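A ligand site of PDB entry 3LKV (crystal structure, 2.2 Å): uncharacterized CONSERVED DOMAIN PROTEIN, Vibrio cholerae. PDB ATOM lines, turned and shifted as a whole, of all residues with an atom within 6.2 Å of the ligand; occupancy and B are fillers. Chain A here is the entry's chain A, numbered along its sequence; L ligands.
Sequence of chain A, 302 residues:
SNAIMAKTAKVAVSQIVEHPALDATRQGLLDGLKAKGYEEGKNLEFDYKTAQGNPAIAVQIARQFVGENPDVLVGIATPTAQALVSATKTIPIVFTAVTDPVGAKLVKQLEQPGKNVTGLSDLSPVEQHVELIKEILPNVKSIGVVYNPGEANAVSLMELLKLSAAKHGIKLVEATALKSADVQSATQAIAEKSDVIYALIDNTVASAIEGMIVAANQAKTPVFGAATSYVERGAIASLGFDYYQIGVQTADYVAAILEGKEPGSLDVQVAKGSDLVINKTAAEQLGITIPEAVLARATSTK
N of Thr 78 lies within hydrogen-bond range of O2 of the ligand (2.8 Å).
O1 of the ligand lies within hydrogen-bond range of N of Thr 99, at 3.0 Å.
The side-chain amide nitrogen (ND2) of Asn 203 lies within hydrogen-bond range of an oxygen (O2) of the ligand (2.9 Å).
The side-chain hydroxyl of Thr 78 sits at hydrogen-bond distance from an oxygen (O1) of the ligand (2.7 Å).
OG1 of Thr 99 sits at hydrogen-bond distance from N1 of the ligand (2.8 Å).
The backbone carbonyl oxygen (O) of Ala 97 lies within hydrogen-bond range of a nitrogen (N1) of the ligand (2.9 Å).
OD2 of Asp 122 lies within salt-bridge range of N1 of the ligand (2.8 Å).
The backbone carbonyl oxygen of Leu 200 is in hydrogen-bond range of the side-chain hydroxyl of Tyr 230, at 2.8 Å.
The side-chain amide nitrogen (ND2) of Asn 153 sits at hydrogen-bond distance from the backbone carbonyl oxygen (O) of Ile 201.
N of Thr 99 sits at hydrogen-bond distance from OD1 of Asp 122 (3.1 Å).
The side-chain carboxylate of Glu 151 lies within hydrogen-bond range of the side-chain amide nitrogen of Asn 153 (3.0 Å).
N of Asp 122 lies within hydrogen-bond range of O of Val 98, at 3.0 Å.
The side-chain carboxylate of Asp 122 is in hydrogen-bond range of the side-chain hydroxyl of Tyr 243, 2.5 Å away.
The backbone NH (N) of Ala 77 is in hydrogen-bond range of the backbone carbonyl oxygen (O) of Thr 96 (3.0 Å).
OD1 of Asn 203 lies within hydrogen-bond range of NE2 of His 19, at 2.9 Å.
CE1 of His 19 touches C7 of the ligand, 3.5 Å away.
CB of Ala 21 touches C8 of the ligand (3.5 Å).
Leu 22 touches the ligand.
CB of Ala 77 touches O2 of the ligand, at 3.4 Å.
Val 98 touches the ligand (CA to O1, 3.5 Å).
CB of Asn 153 touches O1 of the ligand (3.3 Å).
Ile 201 touches the ligand (CG2 to N1, 3.0 Å).
Asp 202 touches the ligand.
CB of Ala 206 touches C7 of the ligand, at 3.9 Å.
OH of Tyr 230 touches C7 of the ligand, 3.7 Å away.
OH of Tyr 243 touches C8 of the ligand, 3.5 Å away.
Hydrophobic or aromatic side chains within 4 Å of the ligand: His 19, Ala 21, Leu 22, Ala 77, Ile 201, Ala 206 and Tyr 243.
Of the 25 residues printed, 16 come within 4 Å of the ligand.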
ATOM      1  N   ILE A  16     -10.984   1.503  -9.612  1.00  0.00           N
ATOM      2  CA  ILE A  16     -11.965   1.227  -8.569  1.00  0.00           C
ATOM      3  C   ILE A  16     -11.808  -0.177  -7.969  1.00  0.00           C
ATOM      4  O   ILE A  16     -11.983  -0.390  -6.746  1.00  0.00           O
ATOM      5  CB  ILE A  16     -13.406   1.539  -9.081  1.00  0.00           C
ATOM      6  CG1 ILE A  16     -14.443   1.368  -7.983  1.00  0.00           C
ATOM      7  CG2 ILE A  16     -13.757   0.716 -10.333  1.00  0.00           C
ATOM      8  CD1 ILE A  16     -14.270   2.235  -6.719  1.00  0.00           C
ATOM      9  N   HIS A  19     -10.957  -5.964 -11.902  1.00  0.00           N
ATOM     10  CA  HIS A  19     -11.655  -6.955 -12.704  1.00  0.00           C
ATOM     11  C   HIS A  19     -11.041  -6.949 -14.094  1.00  0.00           C
ATOM     12  O   HIS A  19     -10.376  -5.984 -14.460  1.00  0.00           O
ATOM     13  CB  HIS A  19     -13.204  -6.764 -12.688  1.00  0.00           C
ATOM     14  CG  HIS A  19     -13.720  -5.474 -13.259  1.00  0.00           C
ATOM     15  ND1 HIS A  19     -13.890  -5.271 -14.609  1.00  0.00           N
ATOM     16  CD2 HIS A  19     -14.226  -4.374 -12.657  1.00  0.00           C
ATOM     17  CE1 HIS A  19     -14.427  -4.079 -14.821  1.00  0.00           C
ATOM     18  NE2 HIS A  19     -14.651  -3.511 -13.641  1.00  0.00           N
ATOM     19  N   ALA A  21     -11.541  -6.407 -17.296  1.00  0.00           N
ATOM     20  CA  ALA A  21     -11.568  -5.280 -18.251  1.00  0.00           C
ATOM     21  C   ALA A  21     -10.667  -4.128 -17.781  1.00  0.00           C
ATOM     22  O   ALA A  21      -9.935  -3.496 -18.583  1.00  0.00           O
ATOM     23  CB  ALA A  21     -12.953  -4.776 -18.512  1.00  0.00           C
ATOM     24  N   LEU A  22     -10.733  -3.814 -16.500  1.00  0.00           N
ATOM     25  CA  LEU A  22      -9.950  -2.669 -16.024  1.00  0.00           C
ATOM     26  C   LEU A  22      -8.476  -2.996 -15.951  1.00  0.00           C
ATOM     27  O   LEU A  22      -7.637  -2.108 -16.204  1.00  0.00           O
ATOM     28  CB  LEU A  22     -10.424  -2.189 -14.689  1.00  0.00           C
ATOM     29  CG  LEU A  22     -11.910  -1.790 -14.669  1.00  0.00           C
ATOM     30  CD1 LEU A  22     -12.190  -1.238 -13.325  1.00  0.00           C
ATOM     31  CD2 LEU A  22     -12.256  -0.794 -15.754  1.00  0.00           C
ATOM     32  N   ILE A  76      -9.088   5.089 -13.837  1.00  0.00           N
ATOM     33  CA  ILE A  76      -9.660   4.033 -14.600  1.00  0.00           C
ATOM     34  C   ILE A  76     -11.001   3.649 -13.893  1.00  0.00           C
ATOM     35  O   ILE A  76     -11.003   3.161 -12.761  1.00  0.00           O
ATOM     36  CB  ILE A  76      -8.747   2.804 -14.621  1.00  0.00           C
ATOM     37  CG1 ILE A  76      -7.399   3.115 -15.238  1.00  0.00           C
ATOM     38  CG2 ILE A  76      -9.415   1.668 -15.352  1.00  0.00           C
ATOM     39  CD1 ILE A  76      -6.390   1.866 -15.224  1.00  0.00           C
ATOM     40  N   ALA A  77     -12.104   3.880 -14.609  1.00  0.00           N
ATOM     41  CA  ALA A  77     -13.475   3.620 -14.148  1.00  0.00           C
ATOM     42  C   ALA A  77     -14.030   4.866 -13.462  1.00  0.00           C
ATOM     43  O   ALA A  77     -13.286   5.726 -12.986  1.00  0.00           O
ATOM     44  CB  ALA A  77     -13.600   2.351 -13.274  1.00  0.00           C
ATOM     45  N   THR A  78     -15.345   4.951 -13.427  1.00  0.00           N
ATOM     46  CA  THR A  78     -16.024   6.193 -13.064  1.00  0.00           C
ATOM     47  C   THR A  78     -15.820   6.647 -11.613  1.00  0.00           C
ATOM     48  O   THR A  78     -15.538   7.823 -11.373  1.00  0.00           O
ATOM     49  CB  THR A  78     -17.541   6.112 -13.422  1.00  0.00           C
ATOM     50  OG1 THR A  78     -17.647   6.091 -14.845  1.00  0.00           O
ATOM     51  CG2 THR A  78     -18.295   7.323 -12.892  1.00  0.00           C
ATOM     52  N   PRO A  79     -15.987   5.737 -10.653  1.00  0.00           N
ATOM     53  CA  PRO A  79     -15.945   6.195  -9.239  1.00  0.00           C
ATOM     54  C   PRO A  79     -14.550   6.698  -8.852  1.00  0.00           C
ATOM     55  O   PRO A  79     -14.430   7.707  -8.169  1.00  0.00           O
ATOM     56  CB  PRO A  79     -16.383   4.969  -8.433  1.00  0.00           C
ATOM     57  CG  PRO A  79     -16.953   4.034  -9.398  1.00  0.00           C
ATOM     58  CD  PRO A  79     -16.371   4.333 -10.773  1.00  0.00           C
ATOM     59  N   THR A  96     -10.300   7.006 -18.059  1.00  0.00           N
ATOM     60  CA  THR A  96     -10.369   5.972 -19.025  1.00  0.00           C
ATOM     61  C   THR A  96     -11.356   4.894 -18.623  1.00  0.00           C
ATOM     62  O   THR A  96     -11.613   4.683 -17.481  1.00  0.00           O
ATOM     63  CB  THR A  96      -8.966   5.444 -19.364  1.00  0.00           C
ATOM     64  OG1 THR A  96      -9.081   4.608 -20.516  1.00  0.00           O
ATOM     65  CG2 THR A  96      -8.294   4.663 -18.204  1.00  0.00           C
ATOM     66  N   ALA A  97     -11.967   4.271 -19.610  1.00  0.00           N
ATOM     67  CA  ALA A  97     -12.995   3.286 -19.438  1.00  0.00           C
ATOM     68  C   ALA A  97     -14.109   3.846 -18.605  1.00  0.00           C
ATOM     69  O   ALA A  97     -14.653   3.174 -17.719  1.00  0.00           O
ATOM     70  CB  ALA A  97     -12.396   1.954 -18.819  1.00  0.00           C
ATOM     71  N   VAL A  98     -14.453   5.106 -18.908  1.00  0.00           N
ATOM     72  CA  VAL A  98     -15.604   5.741 -18.255  1.00  0.00           C
ATOM     73  C   VAL A  98     -16.810   5.784 -19.203  1.00  0.00           C
ATOM     74  O   VAL A  98     -16.736   6.312 -20.335  1.00  0.00           O
ATOM     75  CB  VAL A  98     -15.267   7.146 -17.776  1.00  0.00           C
ATOM     76  CG1 VAL A  98     -16.562   7.927 -17.466  1.00  0.00           C
ATOM     77  CG2 VAL A  98     -14.248   7.071 -16.592  1.00  0.00           C
ATOM     78  N   THR A  99     -17.922   5.232 -18.772  1.00  0.00           N
ATOM     79  CA  THR A  99     -19.072   5.027 -19.624  1.00  0.00           C
ATOM     80  C   THR A  99     -19.677   6.351 -20.136  1.00  0.00           C
ATOM     81  O   THR A  99     -19.902   6.521 -21.350  1.00  0.00           O
ATOM     82  CB  THR A  99     -20.141   4.234 -18.832  1.00  0.00           C
ATOM     83  OG1 THR A  99     -19.718   2.845 -18.710  1.00  0.00           O
ATOM     84  CG2 THR A  99     -21.531   4.392 -19.471  1.00  0.00           C
ATOM     85  N   ASP A 100     -19.904   7.306 -19.236  1.00  0.00           N
ATOM     86  CA  ASP A 100     -20.566   8.602 -19.591  1.00  0.00           C
ATOM     87  C   ASP A 100     -19.988   9.733 -18.742  1.00  0.00           C
ATOM     88  O   ASP A 100     -20.462  10.060 -17.649  1.00  0.00           O
ATOM     89  CB  ASP A 100     -22.050   8.481 -19.358  1.00  0.00           C
ATOM     90  CG  ASP A 100     -22.792   9.803 -19.518  1.00  0.00           C
ATOM     91  OD1 ASP A 100     -22.235  10.771 -20.069  1.00  0.00           O
ATOM     92  OD2 ASP A 100     -23.926   9.881 -19.044  1.00  0.00           O
ATOM     93  N   ASP A 122     -15.976   4.568 -22.680  1.00  0.00           N
ATOM     94  CA  ASP A 122     -16.393   3.224 -23.216  1.00  0.00           C
ATOM     95  C   ASP A 122     -17.912   3.065 -23.239  1.00  0.00           C
ATOM     96  O   ASP A 122     -18.446   2.021 -22.854  1.00  0.00           O
ATOM     97  CB  ASP A 122     -15.773   2.036 -22.461  1.00  0.00           C
ATOM     98  CG  ASP A 122     -16.231   1.950 -20.995  1.00  0.00           C
ATOM     99  OD1 ASP A 122     -16.539   3.020 -20.453  1.00  0.00           O
ATOM    100  OD2 ASP A 122     -16.287   0.835 -20.384  1.00  0.00           O
ATOM    101  N   GLU A 151     -23.246   3.865  -8.861  1.00  0.00           N
ATOM    102  CA  GLU A 151     -22.325   4.072  -9.958  1.00  0.00           C
ATOM    103  C   GLU A 151     -22.945   4.882 -11.093  1.00  0.00           C
ATOM    104  O   GLU A 151     -23.817   4.386 -11.812  1.00  0.00           O
ATOM    105  CB  GLU A 151     -21.873   2.727 -10.510  1.00  0.00           C
ATOM    106  CG  GLU A 151     -20.921   1.925  -9.639  1.00  0.00           C
ATOM    107  CD  GLU A 151     -20.373   0.656 -10.370  1.00  0.00           C
ATOM    108  OE1 GLU A 151     -19.989   0.681 -11.580  1.00  0.00           O
ATOM    109  OE2 GLU A 151     -20.294  -0.375  -9.685  1.00  0.00           O
ATOM    110  N   ASN A 153     -22.008   5.471 -13.950  1.00  0.00           N
ATOM    111  CA  ASN A 153     -22.013   4.723 -15.200  1.00  0.00           C
ATOM    112  C   ASN A 153     -23.234   3.823 -15.352  1.00  0.00           C
ATOM    113  O   ASN A 153     -23.829   3.782 -16.444  1.00  0.00           O
ATOM    114  CB  ASN A 153     -20.760   3.861 -15.408  1.00  0.00           C
ATOM    115  CG  ASN A 153     -20.369   3.147 -14.212  1.00  0.00           C
ATOM    116  OD1 ASN A 153     -20.072   3.787 -13.181  1.00  0.00           O
ATOM    117  ND2 ASN A 153     -20.342   1.813 -14.286  1.00  0.00           N
ATOM    118  N   LEU A 200     -24.493  -5.573 -17.563  1.00  0.00           N
ATOM    119  CA  LEU A 200     -24.002  -4.323 -18.103  1.00  0.00           C
ATOM    120  C   LEU A 200     -22.603  -3.922 -17.614  1.00  0.00           C
ATOM    121  O   LEU A 200     -21.966  -4.602 -16.792  1.00  0.00           O
ATOM    122  CB  LEU A 200     -25.026  -3.199 -17.921  1.00  0.00           C
ATOM    123  CG  LEU A 200     -25.638  -2.883 -16.598  1.00  0.00           C
ATOM    124  CD1 LEU A 200     -24.550  -2.747 -15.708  1.00  0.00           C
ATOM    125  CD2 LEU A 200     -26.449  -1.606 -16.657  1.00  0.00           C
ATOM    126  N   ILE A 201     -22.133  -2.825 -18.196  1.00  0.00           N
ATOM    127  CA  ILE A 201     -20.875  -2.175 -17.848  1.00  0.00           C
ATOM    128  C   ILE A 201     -21.024  -1.465 -16.510  1.00  0.00           C
ATOM    129  O   ILE A 201     -21.227  -0.222 -16.411  1.00  0.00           O
ATOM    130  CB  ILE A 201     -20.429  -1.240 -18.988  1.00  0.00           C
ATOM    131  CG1 ILE A 201     -20.259  -2.056 -20.264  1.00  0.00           C
ATOM    132  CG2 ILE A 201     -19.090  -0.437 -18.658  1.00  0.00           C
ATOM    133  CD1 ILE A 201     -19.241  -3.240 -20.162  1.00  0.00           C
ATOM    134  N   ASP A 202     -20.906  -2.288 -15.482  1.00  0.00           N
ATOM    135  CA  ASP A 202     -21.009  -1.853 -14.102  1.00  0.00           C
ATOM    136  C   ASP A 202     -19.922  -2.610 -13.359  1.00  0.00           C
ATOM    137  O   ASP A 202     -19.830  -3.816 -13.493  1.00  0.00           O
ATOM    138  CB  ASP A 202     -22.405  -2.239 -13.611  1.00  0.00           C
ATOM    139  CG  ASP A 202     -22.612  -2.097 -12.111  1.00  0.00           C
ATOM    140  OD1 ASP A 202     -21.802  -2.643 -11.303  1.00  0.00           O
ATOM    141  OD2 ASP A 202     -23.672  -1.466 -11.744  1.00  0.00           O
ATOM    142  N   ASN A 203     -19.144  -1.902 -12.538  1.00  0.00           N
ATOM    143  CA  ASN A 203     -18.022  -2.503 -11.795  1.00  0.00           C
ATOM    144  C   ASN A 203     -18.410  -3.501 -10.714  1.00  0.00           C
ATOM    145  O   ASN A 203     -17.710  -4.464 -10.467  1.00  0.00           O
ATOM    146  CB  ASN A 203     -17.183  -1.361 -11.171  1.00  0.00           C
ATOM    147  CG  ASN A 203     -16.578  -0.454 -12.242  1.00  0.00           C
ATOM    148  OD1 ASN A 203     -15.680  -0.902 -13.003  1.00  0.00           O
ATOM    149  ND2 ASN A 203     -17.087   0.779 -12.354  1.00  0.00           N
ATOM    150  N   ALA A 206     -19.382  -6.546 -12.728  1.00  0.00           N
ATOM    151  CA  ALA A 206     -18.139  -7.118 -13.258  1.00  0.00           C
ATOM    152  C   ALA A 206     -17.396  -7.884 -12.155  1.00  0.00           C
ATOM    153  O   ALA A 206     -16.894  -8.950 -12.393  1.00  0.00           O
ATOM    154  CB  ALA A 206     -17.227  -6.048 -13.922  1.00  0.00           C
ATOM    155  N   ALA A 227     -19.538  -6.890 -22.043  1.00  0.00           N
ATOM    156  CA  ALA A 227     -18.070  -6.985 -22.013  1.00  0.00           C
ATOM    157  C   ALA A 227     -17.679  -8.404 -22.333  1.00  0.00           C
ATOM    158  O   ALA A 227     -18.298  -9.342 -21.858  1.00  0.00           O
ATOM    159  CB  ALA A 227     -17.522  -6.588 -20.627  1.00  0.00           C
ATOM    160  N   SER A 229     -15.075 -10.013 -21.195  1.00  0.00           N
ATOM    161  CA  SER A 229     -14.726 -10.709 -19.965  1.00  0.00           C
ATOM    162  C   SER A 229     -15.967 -11.472 -19.442  1.00  0.00           C
ATOM    163  O   SER A 229     -15.829 -12.498 -18.794  1.00  0.00           O
ATOM    164  CB  SER A 229     -14.174  -9.734 -18.905  1.00  0.00           C
ATOM    165  OG  SER A 229     -15.063  -8.613 -18.697  1.00  0.00           O
ATOM    166  N   TYR A 230     -17.167 -11.006 -19.743  1.00  0.00           N
ATOM    167  CA  TYR A 230     -18.330 -11.731 -19.231  1.00  0.00           C
ATOM    168  C   TYR A 230     -18.578 -13.062 -19.976  1.00  0.00           C
ATOM    169  O   TYR A 230     -19.011 -14.034 -19.351  1.00  0.00           O
ATOM    170  CB  TYR A 230     -19.569 -10.881 -19.263  1.00  0.00           C
ATOM    171  CG  TYR A 230     -19.509  -9.571 -18.501  1.00  0.00           C
ATOM    172  CD1 TYR A 230     -18.579  -9.335 -17.513  1.00  0.00           C
ATOM    173  CD2 TYR A 230     -20.465  -8.603 -18.724  1.00  0.00           C
ATOM    174  CE1 TYR A 230     -18.548  -8.140 -16.847  1.00  0.00           C
ATOM    175  CE2 TYR A 230     -20.488  -7.415 -18.033  1.00  0.00           C
ATOM    176  CZ  TYR A 230     -19.520  -7.174 -17.108  1.00  0.00           C
ATOM    177  OH  TYR A 230     -19.556  -5.986 -16.446  1.00  0.00           O
ATOM    178  N   TYR A 243     -10.597  -3.587 -24.236  1.00  0.00           N
ATOM    179  CA  TYR A 243     -10.137  -2.662 -23.200  1.00  0.00           C
ATOM    180  C   TYR A 243      -8.605  -2.494 -23.241  1.00  0.00           C
ATOM    181  O   TYR A 243      -8.089  -1.460 -22.822  1.00  0.00           O
ATOM    182  CB  TYR A 243     -10.689  -3.044 -21.809  1.00  0.00           C
ATOM    183  CG  TYR A 243     -12.124  -2.659 -21.680  1.00  0.00           C
ATOM    184  CD1 TYR A 243     -13.146  -3.545 -22.022  1.00  0.00           C
ATOM    185  CD2 TYR A 243     -12.467  -1.404 -21.256  1.00  0.00           C
ATOM    186  CE1 TYR A 243     -14.496  -3.146 -21.921  1.00  0.00           C
ATOM    187  CE2 TYR A 243     -13.777  -0.996 -21.163  1.00  0.00           C
ATOM    188  CZ  TYR A 243     -14.799  -1.843 -21.517  1.00  0.00           C
ATOM    189  OH  TYR A 243     -16.107  -1.428 -21.394  1.00  0.00           O
HETATM  190  N1  LIG L   1     -17.192   1.834 -17.950  1.00  0.00           N
HETATM  191  C1  LIG L   1     -17.149   1.433 -16.502  1.00  0.00           C
HETATM  192  C2  LIG L   1     -17.141   2.717 -15.619  1.00  0.00           C
HETATM  193  O1  LIG L   1     -17.538   3.788 -16.164  1.00  0.00           O
HETATM  194  C3  LIG L   1     -15.967   0.489 -16.188  1.00  0.00           C
HETATM  195  C4  LIG L   1     -16.201  -0.944 -16.666  1.00  0.00           C
HETATM  196  C5  LIG L   1     -17.105  -1.775 -15.985  1.00  0.00           C
HETATM  197  C6  LIG L   1     -15.553  -1.442 -17.771  1.00  0.00           C
HETATM  198  C7  LIG L   1     -17.351  -3.040 -16.414  1.00  0.00           C
HETATM  199  C8  LIG L   1     -15.778  -2.714 -18.206  1.00  0.00           C
HETATM  200  C9  LIG L   1     -16.670  -3.537 -17.544  1.00  0.00           C
HETATM  201  O2  LIG L   1     -16.814   2.728 -14.419  1.00  0.00           O
